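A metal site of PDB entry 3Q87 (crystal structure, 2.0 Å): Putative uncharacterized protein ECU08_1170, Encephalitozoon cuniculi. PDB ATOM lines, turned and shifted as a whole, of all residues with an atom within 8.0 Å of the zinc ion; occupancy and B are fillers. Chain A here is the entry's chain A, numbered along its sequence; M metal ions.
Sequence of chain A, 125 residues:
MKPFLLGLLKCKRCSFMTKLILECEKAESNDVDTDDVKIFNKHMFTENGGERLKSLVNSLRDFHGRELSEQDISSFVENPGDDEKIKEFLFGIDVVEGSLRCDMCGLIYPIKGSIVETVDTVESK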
ATOM      1  N   LYS A  10      23.647  -1.376 -29.101  1.00  0.00           N
ATOM      2  CA  LYS A  10      23.652  -0.009 -29.589  1.00  0.00           C
ATOM      3  C   LYS A  10      22.862   0.888 -28.651  1.00  0.00           C
ATOM      4  O   LYS A  10      22.056   0.405 -27.853  1.00  0.00           O
ATOM      5  CB  LYS A  10      23.064   0.075 -30.994  1.00  0.00           C
ATOM      6  CG  LYS A  10      21.549  -0.160 -31.065  1.00  0.00           C
ATOM      7  CD  LYS A  10      21.039   0.031 -32.490  1.00  0.00           C
ATOM      8  CE  LYS A  10      19.522  -0.022 -32.577  1.00  0.00           C
ATOM      9  NZ  LYS A  10      18.901   1.229 -32.086  1.00  0.00           N
ATOM     10  N   CYS A  11      23.102   2.190 -28.750  1.00  0.00           N
ATOM     11  CA  CYS A  11      22.334   3.146 -27.975  1.00  0.00           C
ATOM     12  C   CYS A  11      20.893   3.102 -28.444  1.00  0.00           C
ATOM     13  O   CYS A  11      20.618   3.089 -29.648  1.00  0.00           O
ATOM     14  CB  CYS A  11      22.882   4.560 -28.142  1.00  0.00           C
ATOM     15  SG  CYS A  11      21.812   5.791 -27.375  1.00  0.00           S
ATOM     16  N   LYS A  12      19.976   3.061 -27.493  1.00  0.00           N
ATOM     17  CA  LYS A  12      18.586   2.849 -27.858  1.00  0.00           C
ATOM     18  C   LYS A  12      17.886   4.171 -28.187  1.00  0.00           C
ATOM     19  O   LYS A  12      16.723   4.183 -28.584  1.00  0.00           O
ATOM     20  CB  LYS A  12      17.846   2.112 -26.742  1.00  0.00           C
ATOM     21  CG  LYS A  12      17.585   2.975 -25.521  1.00  0.00           C
ATOM     22  CD  LYS A  12      16.745   2.238 -24.502  1.00  0.00           C
ATOM     23  CE  LYS A  12      16.636   3.039 -23.214  1.00  0.00           C
ATOM     24  NZ  LYS A  12      15.844   2.264 -22.201  1.00  0.00           N
ATOM     25  N   ARG A  13      18.606   5.278 -28.009  1.00  0.00           N
ATOM     26  CA  ARG A  13      18.033   6.608 -28.227  1.00  0.00           C
ATOM     27  C   ARG A  13      18.531   7.221 -29.552  1.00  0.00           C
ATOM     28  O   ARG A  13      17.735   7.733 -30.342  1.00  0.00           O
ATOM     29  CB  ARG A  13      18.413   7.527 -27.074  1.00  0.00           C
ATOM     30  CG  ARG A  13      18.274   8.999 -27.429  1.00  0.00           C
ATOM     31  CD  ARG A  13      19.084   9.852 -26.466  1.00  0.00           C
ATOM     32  NE  ARG A  13      18.345  10.037 -25.234  1.00  0.00           N
ATOM     33  CZ  ARG A  13      18.895  10.202 -24.038  1.00  0.00           C
ATOM     34  NH1 ARG A  13      20.217  10.215 -23.891  1.00  0.00           N
ATOM     35  NH2 ARG A  13      18.110  10.363 -22.984  1.00  0.00           N
ATOM     36  N   CYS A  14      19.832   7.148 -29.793  1.00  0.00           N
ATOM     37  CA  CYS A  14      20.387   7.603 -31.067  1.00  0.00           C
ATOM     38  C   CYS A  14      19.899   6.716 -32.212  1.00  0.00           C
ATOM     39  O   CYS A  14      19.871   5.500 -32.108  1.00  0.00           O
ATOM     40  CB  CYS A  14      21.916   7.664 -31.000  1.00  0.00           C
ATOM     41  SG  CYS A  14      22.531   8.914 -29.815  1.00  0.00           S
ATOM     42  N   SER A  15      19.482   7.348 -33.309  1.00  0.00           N
ATOM     43  CA  SER A  15      18.864   6.647 -34.428  1.00  0.00           C
ATOM     44  C   SER A  15      19.913   6.225 -35.442  1.00  0.00           C
ATOM     45  O   SER A  15      19.602   5.789 -36.537  1.00  0.00           O
ATOM     46  CB  SER A  15      17.854   7.564 -35.095  1.00  0.00           C
ATOM     47  OG  SER A  15      18.472   8.805 -35.382  1.00  0.00           O
ATOM     48  N   PHE A  16      21.177   6.385 -35.065  1.00  0.00           N
ATOM     49  CA  PHE A  16      22.303   5.988 -35.907  1.00  0.00           C
ATOM     50  C   PHE A  16      23.302   5.297 -34.998  1.00  0.00           C
ATOM     51  O   PHE A  16      23.257   5.482 -33.784  1.00  0.00           O
ATOM     52  CB  PHE A  16      22.945   7.220 -36.539  1.00  0.00           C
ATOM     53  CG  PHE A  16      23.207   8.343 -35.568  1.00  0.00           C
ATOM     54  CD1 PHE A  16      24.496   8.640 -35.141  1.00  0.00           C
ATOM     55  CD2 PHE A  16      22.156   9.080 -35.050  1.00  0.00           C
ATOM     56  CE1 PHE A  16      24.731   9.654 -34.235  1.00  0.00           C
ATOM     57  CE2 PHE A  16      22.380  10.102 -34.147  1.00  0.00           C
ATOM     58  CZ  PHE A  16      23.672  10.395 -33.740  1.00  0.00           C
ATOM     59  N   MET A  17      24.187   4.498 -35.580  1.00  0.00           N
ATOM     60  CA  MET A  17      25.254   3.869 -34.798  1.00  0.00           C
ATOM     61  C   MET A  17      26.134   4.924 -34.131  1.00  0.00           C
ATOM     62  O   MET A  17      26.466   5.941 -34.737  1.00  0.00           O
ATOM     63  CB  MET A  17      26.147   2.970 -35.658  1.00  0.00           C
ATOM     64  CG  MET A  17      25.638   1.557 -35.887  1.00  0.00           C
ATOM     65  SD  MET A  17      25.306   0.609 -34.388  1.00  0.00           S
ATOM     66  CE  MET A  17      23.555   0.866 -34.252  1.00  0.00           C
ATOM     67  N   THR A  18      26.504   4.648 -32.885  1.00  0.00           N
ATOM     68  CA  THR A  18      27.440   5.448 -32.139  1.00  0.00           C
ATOM     69  C   THR A  18      28.365   4.454 -31.449  1.00  0.00           C
ATOM     70  O   THR A  18      28.172   3.242 -31.578  1.00  0.00           O
ATOM     71  CB  THR A  18      26.715   6.251 -31.049  1.00  0.00           C
ATOM     72  OG1 THR A  18      26.105   5.341 -30.136  1.00  0.00           O
ATOM     73  CG2 THR A  18      25.619   7.142 -31.651  1.00  0.00           C
ATOM     74  N   LYS A  19      29.356   4.939 -30.714  1.00  0.00           N
ATOM     75  CA  LYS A  19      30.273   4.053 -29.996  1.00  0.00           C
ATOM     76  C   LYS A  19      29.863   3.941 -28.542  1.00  0.00           C
ATOM     77  O   LYS A  19      29.681   4.951 -27.873  1.00  0.00           O
ATOM     78  CB  LYS A  19      31.689   4.609 -30.056  1.00  0.00           C
ATOM     79  CG  LYS A  19      32.236   4.790 -31.452  1.00  0.00           C
ATOM     80  CD  LYS A  19      33.436   5.722 -31.423  1.00  0.00           C
ATOM     81  CE  LYS A  19      33.702   6.362 -32.789  1.00  0.00           C
ATOM     82  NZ  LYS A  19      34.770   7.393 -32.707  1.00  0.00           N
ATOM     83  N   LEU A  20      29.695   2.713 -28.044  1.00  0.00           N
ATOM     84  CA  LEU A  20      29.432   2.518 -26.623  1.00  0.00           C
ATOM     85  C   LEU A  20      30.759   2.347 -25.902  1.00  0.00           C
ATOM     86  O   LEU A  20      31.516   1.443 -26.235  1.00  0.00           O
ATOM     87  CB  LEU A  20      28.533   1.297 -26.383  1.00  0.00           C
ATOM     88  CG  LEU A  20      27.174   1.348 -27.116  1.00  0.00           C
ATOM     89  CD1 LEU A  20      26.288   0.152 -26.765  1.00  0.00           C
ATOM     90  CD2 LEU A  20      26.476   2.681 -26.828  1.00  0.00           C
ATOM     91  N   ARG A 101      28.586   3.563 -22.063  1.00  0.00           N
ATOM     92  CA  ARG A 101      28.122   4.931 -22.303  1.00  0.00           C
ATOM     93  C   ARG A 101      28.141   5.269 -23.800  1.00  0.00           C
ATOM     94  O   ARG A 101      29.157   5.127 -24.452  1.00  0.00           O
ATOM     95  CB  ARG A 101      29.007   5.927 -21.531  1.00  0.00           C
ATOM     96  CG  ARG A 101      28.679   7.408 -21.845  1.00  0.00           C
ATOM     97  CD  ARG A 101      29.475   8.398 -21.003  1.00  0.00           C
ATOM     98  NE  ARG A 101      30.896   8.066 -20.937  1.00  0.00           N
ATOM     99  CZ  ARG A 101      31.779   8.349 -21.889  1.00  0.00           C
ATOM    100  NH1 ARG A 101      31.379   8.948 -23.008  1.00  0.00           N
ATOM    101  NH2 ARG A 101      33.058   8.018 -21.742  1.00  0.00           N
ATOM    102  N   CYS A 102      27.005   5.727 -24.333  1.00  0.00           N
ATOM    103  CA  CYS A 102      26.939   6.196 -25.704  1.00  0.00           C
ATOM    104  C   CYS A 102      27.769   7.460 -25.850  1.00  0.00           C
ATOM    105  O   CYS A 102      27.558   8.415 -25.134  1.00  0.00           O
ATOM    106  CB  CYS A 102      25.497   6.528 -26.093  1.00  0.00           C
ATOM    107  SG  CYS A 102      25.372   7.318 -27.754  1.00  0.00           S
ATOM    108  N   ASP A 103      28.720   7.458 -26.777  1.00  0.00           N
ATOM    109  CA  ASP A 103      29.619   8.595 -26.928  1.00  0.00           C
ATOM    110  C   ASP A 103      28.922   9.824 -27.506  1.00  0.00           C
ATOM    111  O   ASP A 103      29.450  10.922 -27.407  1.00  0.00           O
ATOM    112  CB  ASP A 103      30.850   8.243 -27.763  1.00  0.00           C
ATOM    113  CG  ASP A 103      30.522   7.963 -29.221  1.00  0.00           C
ATOM    114  OD1 ASP A 103      29.323   7.819 -29.561  1.00  0.00           O
ATOM    115  OD2 ASP A 103      31.453   7.867 -30.050  1.00  0.00           O
ATOM    116  N   MET A 104      27.737   9.649 -28.085  1.00  0.00           N
ATOM    117  CA  MET A 104      27.047  10.779 -28.693  1.00  0.00           C
ATOM    118  C   MET A 104      26.043  11.465 -27.766  1.00  0.00           C
ATOM    119  O   MET A 104      26.006  12.700 -27.698  1.00  0.00           O
ATOM    120  CB  MET A 104      26.369  10.399 -30.010  1.00  0.00           C
ATOM    121  CG  MET A 104      27.355   9.993 -31.108  1.00  0.00           C
ATOM    122  SD  MET A 104      28.350  11.380 -31.728  1.00  0.00           S
ATOM    123  CE  MET A 104      27.028  12.494 -32.224  1.00  0.00           C
ATOM    124  N   CYS A 105      25.219  10.681 -27.066  1.00  0.00           N
ATOM    125  CA  CYS A 105      24.194  11.295 -26.221  1.00  0.00           C
ATOM    126  C   CYS A 105      24.465  11.081 -24.735  1.00  0.00           C
ATOM    127  O   CYS A 105      23.739  11.603 -23.898  1.00  0.00           O
ATOM    128  CB  CYS A 105      22.817  10.758 -26.571  1.00  0.00           C
ATOM    129  SG  CYS A 105      22.561   9.087 -25.937  1.00  0.00           S
ATOM    130  N   GLY A 106      25.508  10.309 -24.412  1.00  0.00           N
ATOM    131  CA  GLY A 106      25.846  10.052 -23.010  1.00  0.00           C
ATOM    132  C   GLY A 106      24.946   9.091 -22.234  1.00  0.00           C
ATOM    133  O   GLY A 106      25.128   8.905 -21.045  1.00  0.00           O
ATOM    134  N   LEU A 107      23.961   8.499 -22.895  1.00  0.00           N
ATOM    135  CA  LEU A 107      23.125   7.485 -22.254  1.00  0.00           C
ATOM    136  C   LEU A 107      23.991   6.359 -21.671  1.00  0.00           C
ATOM    137  O   LEU A 107      24.938   5.886 -22.298  1.00  0.00           O
ATOM    138  CB  LEU A 107      22.132   6.891 -23.256  1.00  0.00           C
ATOM    139  CG  LEU A 107      21.099   5.918 -22.705  1.00  0.00           C
ATOM    140  CD1 LEU A 107      20.042   6.687 -21.936  1.00  0.00           C
ATOM    141  CD2 LEU A 107      20.454   5.112 -23.818  1.00  0.00           C
ATOM    142  N   ILE A 108      23.645   5.924 -20.462  1.00  0.00           N
ATOM    143  CA  ILE A 108      24.407   4.908 -19.741  1.00  0.00           C
ATOM    144  C   ILE A 108      23.620   3.625 -19.513  1.00  0.00           C
ATOM    145  O   ILE A 108      22.510   3.669 -18.980  1.00  0.00           O
ATOM    146  CB  ILE A 108      24.774   5.388 -18.327  1.00  0.00           C
ATOM    147  CG1 ILE A 108      25.575   6.694 -18.362  1.00  0.00           C
ATOM    148  CG2 ILE A 108      25.524   4.294 -17.582  1.00  0.00           C
ATOM    149  CD1 ILE A 108      26.937   6.532 -18.905  1.00  0.00           C
ATOM    150  N   TYR A 109      24.219   2.507 -19.900  1.00  0.00           N
ATOM    151  CA  TYR A 109      23.730   1.177 -19.565  1.00  0.00           C
ATOM    152  C   TYR A 109      24.593   0.601 -18.432  1.00  0.00           C
ATOM    153  O   TYR A 109      25.731   0.210 -18.635  1.00  0.00           O
ATOM    154  CB  TYR A 109      23.848   0.222 -20.759  1.00  0.00           C
ATOM    155  CG  TYR A 109      23.035   0.541 -22.009  1.00  0.00           C
ATOM    156  CD1 TYR A 109      21.868   1.278 -21.952  1.00  0.00           C
ATOM    157  CD2 TYR A 109      23.442   0.040 -23.249  1.00  0.00           C
ATOM    158  CE1 TYR A 109      21.132   1.536 -23.095  1.00  0.00           C
ATOM    159  CE2 TYR A 109      22.717   0.298 -24.401  1.00  0.00           C
ATOM    160  CZ  TYR A 109      21.568   1.032 -24.320  1.00  0.00           C
ATOM    161  OH  TYR A 109      20.844   1.262 -25.456  1.00  0.00           O
ATOM    162  N   GLU A 123      21.514   9.034 -17.261  1.00  0.00           N
ATOM    163  CA  GLU A 123      22.023  10.099 -18.117  1.00  0.00           C
ATOM    164  C   GLU A 123      23.348  10.630 -17.578  1.00  0.00           C
ATOM    165  O   GLU A 123      23.531  10.715 -16.371  1.00  0.00           O
ATOM    166  CB  GLU A 123      21.025  11.255 -18.160  1.00  0.00           C
ATOM    167  CG  GLU A 123      19.656  10.879 -18.675  1.00  0.00           C
ATOM    168  CD  GLU A 123      19.685  10.426 -20.117  1.00  0.00           C
ATOM    169  OE1 GLU A 123      20.641  10.788 -20.837  1.00  0.00           O
ATOM    170  OE2 GLU A 123      18.748   9.708 -20.529  1.00  0.00           O
ATOM    171  N   LYS A 125      24.971  13.312 -19.524  1.00  0.00           N
ATOM    172  CA  LYS A 125      25.127  14.640 -20.126  1.00  0.00           C
ATOM    173  C   LYS A 125      24.150  15.641 -19.515  1.00  0.00           C
ATOM    174  O   LYS A 125      23.484  15.353 -18.508  1.00  0.00           O
ATOM    175  CB  LYS A 125      25.002  14.573 -21.657  1.00  0.00           C
ATOM    176  CG  LYS A 125      26.205  13.912 -22.332  1.00  0.00           C
ATOM    177  CD  LYS A 125      26.246  14.233 -23.823  1.00  0.00           C
ATOM    178  CE  LYS A 125      27.455  13.603 -24.502  1.00  0.00           C
ATOM    179  NZ  LYS A 125      27.552  13.991 -25.946  1.00  0.00           N
ATOM    180  OXT LYS A 125      24.005  16.773 -20.010  1.00  0.00           O
HETATM  181 ZN    ZN M   1      23.109   7.725 -27.758  1.00  0.00          ZN
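The zinc ion is bound by the side-chain sulfur of Cys 102, the side-chain sulfur of Cys 105, the side-chain sulfur of Cys 11 and the side-chain sulfur of Cys 14.
The side-chain sulfur (SG) of Cys 102 sits close to the side-chain hydroxyl (OG1) of Thr 18, at 3.2 Å.
N of Cys 102 is in hydrogen-bond range of O of Leu 107 (2.9 Å).
The side-chain sulfur (SG) of Cys 102 sits close to the backbone NH (N) of Met 104, 3.3 Å away.
SG of Cys 105 sits close to N of Leu 107 (3.4 Å).
NH1 of Arg 13 sits close to SG of Cys 105, at 3.3 Å.
N of Arg 13 sits close to SG of Cys 11, 3.3 Å away.
The nearest printed residue that does not touch the zinc ion is Thr 18 (4.5 Å).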
